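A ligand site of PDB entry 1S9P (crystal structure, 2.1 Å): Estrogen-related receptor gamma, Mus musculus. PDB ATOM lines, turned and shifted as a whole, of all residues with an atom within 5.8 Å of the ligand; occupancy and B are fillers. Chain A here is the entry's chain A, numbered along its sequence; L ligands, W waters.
Water W1 lies within hydrogen-bond range of OE1 of Glu 44 (2.5 Å), O of Leu 78 (2.9 Å), O2 of the ligand (2.9 Å) and NH2 of Arg 85 (3.2 Å).
Residues that only touch the ligand: Leu 34 (3.9 Å), Leu 37 (3.7 Å), Ala 41 (3.4 Å), Met 75 (3.7 Å), Leu 78 (3.5 Å), Val 82 (3.5 Å), Arg 85 (3.9 Å), Tyr 95 (3.0 Å), Leu 114 (3.9 Å), Ala 200 (3.7 Å), Phe 204 (3.4 Å) and Ile 207 (3.2 Å). Hydrophobic or aromatic side chains that line the ligand: Leu 34, Leu 37, Ala 41, Met 75, Leu 78, Val 82, Tyr 95, Leu 114, His 203, Phe 204 and Ile 207.
The guanidinium group (NH2) of Arg 85 is in salt-bridge range of the side-chain carboxylate (OE1) of Glu 44 (3.9 Å). The guanidinium group of Arg 85 lies within hydrogen-bond range of the backbone carbonyl oxygen of Tyr 95, at 3.0 Å. The side-chain amide oxygen (OD1) of Asn 115 is in hydrogen-bond range of the side-chain hydroxyl (OH) of Tyr 95, at 2.7 Å. The backbone carbonyl oxygen (O) of Leu 34 sits at hydrogen-bond distance from the side-chain sulfur (SG) of Cys 38 (3.3 Å).
OE2 of Glu 44 sits at hydrogen-bond distance from O2 of the ligand (2.5 Å). An oxygen (O1) of the ligand sits close to the backbone carbonyl oxygen (O) of His 203 (3.4 Å). A ring nitrogen (ND1) of His 203 sits at hydrogen-bond distance from an oxygen (O1) of the ligand (2.6 Å).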
ATOM      1  N   LEU A  34      27.196   3.102 -26.519  1.00  0.00           N
ATOM      2  CA  LEU A  34      26.127   3.748 -25.772  1.00  0.00           C
ATOM      3  C   LEU A  34      24.885   2.851 -25.665  1.00  0.00           C
ATOM      4  O   LEU A  34      24.255   2.780 -24.608  1.00  0.00           O
ATOM      5  CB  LEU A  34      25.767   5.070 -26.432  1.00  0.00           C
ATOM      6  CG  LEU A  34      26.900   6.102 -26.525  1.00  0.00           C
ATOM      7  CD1 LEU A  34      26.436   7.292 -27.334  1.00  0.00           C
ATOM      8  CD2 LEU A  34      27.333   6.529 -25.122  1.00  0.00           C
ATOM      9  N   LEU A  37      25.764   0.223 -23.114  1.00  0.00           N
ATOM     10  CA  LEU A  37      25.796   0.747 -21.756  1.00  0.00           C
ATOM     11  C   LEU A  37      24.388   0.978 -21.227  1.00  0.00           C
ATOM     12  O   LEU A  37      24.114   0.721 -20.064  1.00  0.00           O
ATOM     13  CB  LEU A  37      26.615   2.049 -21.714  1.00  0.00           C
ATOM     14  CG  LEU A  37      28.127   1.860 -21.930  1.00  0.00           C
ATOM     15  CD1 LEU A  37      28.829   3.200 -21.992  1.00  0.00           C
ATOM     16  CD2 LEU A  37      28.697   1.023 -20.778  1.00  0.00           C
ATOM     17  N   CYS A  38      23.503   1.450 -22.099  1.00  0.00           N
ATOM     18  CA  CYS A  38      22.122   1.715 -21.695  1.00  0.00           C
ATOM     19  C   CYS A  38      21.353   0.435 -21.408  1.00  0.00           C
ATOM     20  O   CYS A  38      20.507   0.406 -20.513  1.00  0.00           O
ATOM     21  CB  CYS A  38      21.390   2.528 -22.764  1.00  0.00           C
ATOM     22  SG  CYS A  38      21.929   4.256 -22.846  1.00  0.00           S
ATOM     23  N   LEU A  40      22.729  -2.372 -20.402  1.00  0.00           N
ATOM     24  CA  LEU A  40      23.322  -2.875 -19.171  1.00  0.00           C
ATOM     25  C   LEU A  40      22.663  -2.151 -17.992  1.00  0.00           C
ATOM     26  O   LEU A  40      22.112  -2.775 -17.084  1.00  0.00           O
ATOM     27  CB  LEU A  40      24.832  -2.618 -19.162  1.00  0.00           C
ATOM     28  CG  LEU A  40      25.570  -2.834 -17.842  1.00  0.00           C
ATOM     29  CD1 LEU A  40      25.407  -4.277 -17.382  1.00  0.00           C
ATOM     30  CD2 LEU A  40      27.030  -2.489 -18.004  1.00  0.00           C
ATOM     31  N   ALA A  41      22.708  -0.829 -18.027  1.00  0.00           N
ATOM     32  CA  ALA A  41      22.120  -0.031 -16.961  1.00  0.00           C
ATOM     33  C   ALA A  41      20.658  -0.386 -16.755  1.00  0.00           C
ATOM     34  O   ALA A  41      20.198  -0.503 -15.617  1.00  0.00           O
ATOM     35  CB  ALA A  41      22.245   1.431 -17.277  1.00  0.00           C
ATOM     36  N   GLU A  44      20.550  -3.408 -14.850  1.00  0.00           N
ATOM     37  CA  GLU A  44      21.035  -3.198 -13.482  1.00  0.00           C
ATOM     38  C   GLU A  44      19.959  -2.507 -12.648  1.00  0.00           C
ATOM     39  O   GLU A  44      19.803  -2.781 -11.460  1.00  0.00           O
ATOM     40  CB  GLU A  44      22.290  -2.339 -13.451  1.00  0.00           C
ATOM     41  CG  GLU A  44      23.523  -3.000 -14.036  1.00  0.00           C
ATOM     42  CD  GLU A  44      24.755  -2.133 -13.885  1.00  0.00           C
ATOM     43  OE1 GLU A  44      25.438  -2.222 -12.853  1.00  0.00           O
ATOM     44  OE2 GLU A  44      25.043  -1.345 -14.808  1.00  0.00           O
ATOM     45  N   TRP A  74      19.506   6.317  -8.247  1.00  0.00           N
ATOM     46  CA  TRP A  74      19.920   5.157  -9.066  1.00  0.00           C
ATOM     47  C   TRP A  74      21.280   5.344  -9.749  1.00  0.00           C
ATOM     48  O   TRP A  74      22.056   4.395  -9.807  1.00  0.00           O
ATOM     49  CB  TRP A  74      18.838   4.785 -10.073  1.00  0.00           C
ATOM     50  CG  TRP A  74      18.618   5.796 -11.174  1.00  0.00           C
ATOM     51  CD1 TRP A  74      17.723   6.813 -11.149  1.00  0.00           C
ATOM     52  CD2 TRP A  74      19.282   5.876 -12.457  1.00  0.00           C
ATOM     53  NE1 TRP A  74      17.778   7.530 -12.309  1.00  0.00           N
ATOM     54  CE2 TRP A  74      18.725   6.982 -13.137  1.00  0.00           C
ATOM     55  CE3 TRP A  74      20.296   5.135 -13.080  1.00  0.00           C
ATOM     56  CZ2 TRP A  74      19.138   7.347 -14.425  1.00  0.00           C
ATOM     57  CZ3 TRP A  74      20.700   5.508 -14.362  1.00  0.00           C
ATOM     58  CH2 TRP A  74      20.125   6.612 -15.017  1.00  0.00           C
ATOM     59  N   MET A  75      21.557   6.540 -10.271  1.00  0.00           N
ATOM     60  CA  MET A  75      22.835   6.743 -10.955  1.00  0.00           C
ATOM     61  C   MET A  75      24.037   6.688 -10.003  1.00  0.00           C
ATOM     62  O   MET A  75      25.105   6.231 -10.378  1.00  0.00           O
ATOM     63  CB  MET A  75      22.813   8.067 -11.725  1.00  0.00           C
ATOM     64  CG  MET A  75      24.055   8.303 -12.546  1.00  0.00           C
ATOM     65  SD  MET A  75      24.361   7.026 -13.776  1.00  0.00           S
ATOM     66  CE  MET A  75      23.393   7.654 -15.155  1.00  0.00           C
ATOM     67  N   LEU A  78      24.604   2.977  -9.469  1.00  0.00           N
ATOM     68  CA  LEU A  78      25.246   2.377 -10.639  1.00  0.00           C
ATOM     69  C   LEU A  78      26.725   2.766 -10.704  1.00  0.00           C
ATOM     70  O   LEU A  78      27.599   1.931 -10.860  1.00  0.00           O
ATOM     71  CB  LEU A  78      24.554   2.821 -11.920  1.00  0.00           C
ATOM     72  CG  LEU A  78      23.132   2.331 -12.219  1.00  0.00           C
ATOM     73  CD1 LEU A  78      22.739   2.779 -13.626  1.00  0.00           C
ATOM     74  CD2 LEU A  78      23.067   0.812 -12.109  1.00  0.00           C
ATOM     75  N   ILE A  79      27.006   4.070 -10.584  1.00  0.00           N
ATOM     76  CA  ILE A  79      28.390   4.558 -10.622  1.00  0.00           C
ATOM     77  C   ILE A  79      29.279   3.959  -9.525  1.00  0.00           C
ATOM     78  O   ILE A  79      30.403   3.558  -9.780  1.00  0.00           O
ATOM     79  CB  ILE A  79      28.439   6.109 -10.506  1.00  0.00           C
ATOM     80  CG1 ILE A  79      27.842   6.760 -11.760  1.00  0.00           C
ATOM     81  CG2 ILE A  79      29.884   6.566 -10.291  1.00  0.00           C
ATOM     82  CD1 ILE A  79      28.621   6.507 -13.026  1.00  0.00           C
ATOM     83  N   VAL A  82      30.355   0.581 -10.616  1.00  0.00           N
ATOM     84  CA  VAL A  82      31.426   0.645 -11.615  1.00  0.00           C
ATOM     85  C   VAL A  82      32.736   0.992 -10.950  1.00  0.00           C
ATOM     86  O   VAL A  82      33.769   0.359 -11.206  1.00  0.00           O
ATOM     87  CB  VAL A  82      31.129   1.694 -12.707  1.00  0.00           C
ATOM     88  CG1 VAL A  82      32.284   1.766 -13.687  1.00  0.00           C
ATOM     89  CG2 VAL A  82      29.862   1.329 -13.429  1.00  0.00           C
ATOM     90  N   ARG A  85      34.202  -1.935  -8.934  1.00  0.00           N
ATOM     91  CA  ARG A  85      34.703  -2.990  -9.822  1.00  0.00           C
ATOM     92  C   ARG A  85      35.991  -2.576 -10.533  1.00  0.00           C
ATOM     93  O   ARG A  85      36.709  -3.434 -11.077  1.00  0.00           O
ATOM     94  CB  ARG A  85      33.655  -3.342 -10.873  1.00  0.00           C
ATOM     95  CG  ARG A  85      32.366  -3.996 -10.344  1.00  0.00           C
ATOM     96  CD  ARG A  85      31.537  -4.553 -11.488  1.00  0.00           C
ATOM     97  NE  ARG A  85      30.924  -3.498 -12.311  1.00  0.00           N
ATOM     98  CZ  ARG A  85      29.802  -2.842 -11.996  1.00  0.00           C
ATOM     99  NH1 ARG A  85      29.158  -3.118 -10.861  1.00  0.00           N
ATOM    100  NH2 ARG A  85      29.319  -1.931 -12.825  1.00  0.00           N
ATOM    101  N   TYR A  95      32.640  -1.653 -16.409  1.00  0.00           N
ATOM    102  CA  TYR A  95      31.184  -1.528 -16.410  1.00  0.00           C
ATOM    103  C   TYR A  95      30.596  -2.920 -16.180  1.00  0.00           C
ATOM    104  O   TYR A  95      29.559  -3.076 -15.543  1.00  0.00           O
ATOM    105  CB  TYR A  95      30.715  -0.927 -17.728  1.00  0.00           C
ATOM    106  CG  TYR A  95      30.830   0.583 -17.732  1.00  0.00           C
ATOM    107  CD1 TYR A  95      29.894   1.377 -17.065  1.00  0.00           C
ATOM    108  CD2 TYR A  95      31.933   1.216 -18.316  1.00  0.00           C
ATOM    109  CE1 TYR A  95      30.049   2.756 -16.981  1.00  0.00           C
ATOM    110  CE2 TYR A  95      32.090   2.609 -18.233  1.00  0.00           C
ATOM    111  CZ  TYR A  95      31.143   3.369 -17.566  1.00  0.00           C
ATOM    112  OH  TYR A  95      31.294   4.736 -17.471  1.00  0.00           O
ATOM    113  N   LEU A 111      32.843   9.236 -24.352  1.00  0.00           N
ATOM    114  CA  LEU A 111      32.674   9.182 -22.910  1.00  0.00           C
ATOM    115  C   LEU A 111      33.957   9.491 -22.164  1.00  0.00           C
ATOM    116  O   LEU A 111      34.090   9.184 -20.982  1.00  0.00           O
ATOM    117  CB  LEU A 111      32.165   7.792 -22.511  1.00  0.00           C
ATOM    118  CG  LEU A 111      30.727   7.497 -22.951  1.00  0.00           C
ATOM    119  CD1 LEU A 111      30.523   5.998 -23.069  1.00  0.00           C
ATOM    120  CD2 LEU A 111      29.766   8.116 -21.934  1.00  0.00           C
ATOM    121  N   LEU A 114      33.344  12.035 -19.109  1.00  0.00           N
ATOM    122  CA  LEU A 114      32.605  11.353 -18.059  1.00  0.00           C
ATOM    123  C   LEU A 114      33.412  10.213 -17.441  1.00  0.00           C
ATOM    124  O   LEU A 114      33.497  10.101 -16.219  1.00  0.00           O
ATOM    125  CB  LEU A 114      31.281  10.840 -18.618  1.00  0.00           C
ATOM    126  CG  LEU A 114      30.385  10.119 -17.620  1.00  0.00           C
ATOM    127  CD1 LEU A 114      30.132  11.037 -16.415  1.00  0.00           C
ATOM    128  CD2 LEU A 114      29.085   9.734 -18.298  1.00  0.00           C
ATOM    129  N   ASN A 115      34.022   9.372 -18.277  1.00  0.00           N
ATOM    130  CA  ASN A 115      34.808   8.262 -17.737  1.00  0.00           C
ATOM    131  C   ASN A 115      36.005   8.749 -16.951  1.00  0.00           C
ATOM    132  O   ASN A 115      36.413   8.102 -15.994  1.00  0.00           O
ATOM    133  CB  ASN A 115      35.231   7.293 -18.839  1.00  0.00           C
ATOM    134  CG  ASN A 115      34.105   6.380 -19.256  1.00  0.00           C
ATOM    135  OD1 ASN A 115      33.036   6.369 -18.630  1.00  0.00           O
ATOM    136  ND2 ASN A 115      34.319   5.603 -20.313  1.00  0.00           N
ATOM    137  N   ILE A 118      34.649   9.699 -13.577  1.00  0.00           N
ATOM    138  CA  ILE A 118      34.414   8.490 -12.789  1.00  0.00           C
ATOM    139  C   ILE A 118      35.753   7.931 -12.284  1.00  0.00           C
ATOM    140  O   ILE A 118      35.828   7.387 -11.175  1.00  0.00           O
ATOM    141  CB  ILE A 118      33.634   7.439 -13.618  1.00  0.00           C
ATOM    142  CG1 ILE A 118      32.221   7.958 -13.897  1.00  0.00           C
ATOM    143  CG2 ILE A 118      33.558   6.109 -12.871  1.00  0.00           C
ATOM    144  CD1 ILE A 118      31.461   7.160 -14.948  1.00  0.00           C
ATOM    145  N   ALA A 200      26.840  12.439 -15.154  1.00  0.00           N
ATOM    146  CA  ALA A 200      26.471  11.266 -15.951  1.00  0.00           C
ATOM    147  C   ALA A 200      25.039  11.389 -16.428  1.00  0.00           C
ATOM    148  O   ALA A 200      24.734  11.121 -17.602  1.00  0.00           O
ATOM    149  CB  ALA A 200      26.648   9.987 -15.140  1.00  0.00           C
ATOM    150  N   VAL A 201      24.144  11.781 -15.526  1.00  0.00           N
ATOM    151  CA  VAL A 201      22.743  11.921 -15.865  1.00  0.00           C
ATOM    152  C   VAL A 201      22.566  12.962 -16.976  1.00  0.00           C
ATOM    153  O   VAL A 201      21.795  12.757 -17.912  1.00  0.00           O
ATOM    154  CB  VAL A 201      21.887  12.330 -14.628  1.00  0.00           C
ATOM    155  CG1 VAL A 201      20.490  12.704 -15.052  1.00  0.00           C
ATOM    156  CG2 VAL A 201      21.838  11.179 -13.639  1.00  0.00           C
ATOM    157  N   HIS A 203      24.702  13.745 -19.157  1.00  0.00           N
ATOM    158  CA  HIS A 203      25.293  13.217 -20.379  1.00  0.00           C
ATOM    159  C   HIS A 203      24.275  12.280 -21.043  1.00  0.00           C
ATOM    160  O   HIS A 203      24.080  12.332 -22.266  1.00  0.00           O
ATOM    161  CB  HIS A 203      26.574  12.461 -20.039  1.00  0.00           C
ATOM    162  CG  HIS A 203      27.442  12.139 -21.252  1.00  0.00           C
ATOM    163  ND1 HIS A 203      27.104  11.185 -22.188  1.00  0.00           N
ATOM    164  CD2 HIS A 203      28.637  12.647 -21.644  1.00  0.00           C
ATOM    165  CE1 HIS A 203      28.051  11.122 -23.107  1.00  0.00           C
ATOM    166  NE2 HIS A 203      28.994  11.994 -22.795  1.00  0.00           N
ATOM    167  N   PHE A 204      23.666  11.439 -20.222  1.00  0.00           N
ATOM    168  CA  PHE A 204      22.667  10.480 -20.661  1.00  0.00           C
ATOM    169  C   PHE A 204      21.473  11.198 -21.275  1.00  0.00           C
ATOM    170  O   PHE A 204      20.611  10.569 -21.915  1.00  0.00           O
ATOM    171  CB  PHE A 204      22.215   9.666 -19.473  1.00  0.00           C
ATOM    172  CG  PHE A 204      21.188   8.610 -19.779  1.00  0.00           C
ATOM    173  CD1 PHE A 204      21.403   7.642 -20.754  1.00  0.00           C
ATOM    174  CD2 PHE A 204      19.985   8.588 -19.061  1.00  0.00           C
ATOM    175  CE1 PHE A 204      20.443   6.663 -21.002  1.00  0.00           C
ATOM    176  CE2 PHE A 204      19.033   7.616 -19.308  1.00  0.00           C
ATOM    177  CZ  PHE A 204      19.261   6.646 -20.278  1.00  0.00           C
ATOM    178  N   TYR A 205      21.400  12.534 -21.098  1.00  0.00           N
ATOM    179  CA  TYR A 205      20.288  13.361 -21.611  1.00  0.00           C
ATOM    180  C   TYR A 205      20.731  14.102 -22.888  1.00  0.00           C
ATOM    181  O   TYR A 205      19.922  14.229 -23.823  1.00  0.00           O
ATOM    182  CB  TYR A 205      19.797  14.395 -20.576  1.00  0.00           C
ATOM    183  CG  TYR A 205      18.742  13.923 -19.554  1.00  0.00           C
ATOM    184  CD1 TYR A 205      18.323  12.599 -19.594  1.00  0.00           C
ATOM    185  CD2 TYR A 205      18.185  14.783 -18.616  1.00  0.00           C
ATOM    186  CE1 TYR A 205      17.420  12.127 -18.689  1.00  0.00           C
ATOM    187  CE2 TYR A 205      17.252  14.294 -17.698  1.00  0.00           C
ATOM    188  CZ  TYR A 205      16.893  12.964 -17.736  1.00  0.00           C
ATOM    189  OH  TYR A 205      16.001  12.477 -16.824  1.00  0.00           O
ATOM    190  N   ILE A 207      22.433  12.967 -25.061  1.00  0.00           N
ATOM    191  CA  ILE A 207      22.477  11.917 -26.100  1.00  0.00           C
ATOM    192  C   ILE A 207      21.088  11.285 -26.354  1.00  0.00           C
ATOM    193  O   ILE A 207      20.705  11.071 -27.511  1.00  0.00           O
ATOM    194  CB  ILE A 207      23.491  10.769 -25.749  1.00  0.00           C
ATOM    195  CG1 ILE A 207      23.012   9.943 -24.569  1.00  0.00           C
ATOM    196  CG2 ILE A 207      24.859  11.371 -25.465  1.00  0.00           C
ATOM    197  CD1 ILE A 207      22.535   8.553 -24.966  1.00  0.00           C
HETATM  198  C1  LIG L   1      22.832   4.418 -18.676  1.00  0.00           C
HETATM  199  C2  LIG L   1      23.860   5.094 -17.830  1.00  0.00           C
HETATM  200  C3  LIG L   1      25.261   5.267 -18.463  1.00  0.00           C
HETATM  201  C4  LIG L   1      25.303   6.350 -19.563  1.00  0.00           C
HETATM  202  C5  LIG L   1      25.622   7.713 -19.254  1.00  0.00           C
HETATM  203  C6  LIG L   1      25.675   8.701 -20.282  1.00  0.00           C
HETATM  204  C7  LIG L   1      25.405   8.334 -21.623  1.00  0.00           C
HETATM  205  O1  LIG L   1      25.441   9.253 -22.658  1.00  0.00           O
HETATM  206  C8  LIG L   1      25.092   6.989 -21.964  1.00  0.00           C
HETATM  207  C9  LIG L   1      25.047   6.021 -20.936  1.00  0.00           C
HETATM  208  C10 LIG L   1      26.361   4.584 -18.094  1.00  0.00           C
HETATM  209  C11 LIG L   1      26.396   3.493 -16.997  1.00  0.00           C
HETATM  210  C12 LIG L   1      26.065   2.144 -17.312  1.00  0.00           C
HETATM  211  C13 LIG L   1      26.099   1.123 -16.301  1.00  0.00           C
HETATM  212  C14 LIG L   1      26.471   1.456 -14.972  1.00  0.00           C
HETATM  213  O2  LIG L   1      26.523   0.510 -13.975  1.00  0.00           O
HETATM  214  C15 LIG L   1      26.807   2.806 -14.632  1.00  0.00           C
HETATM  215  C16 LIG L   1      26.762   3.813 -15.657  1.00  0.00           C
HETATM  216  C17 LIG L   1      27.768   4.779 -18.717  1.00  0.00           C
HETATM  217  C18 LIG L   1      28.604   5.863 -18.067  1.00  0.00           C
HETATM  218  O   HOH W   1      26.737  -0.738 -11.376  1.00  0.00           O
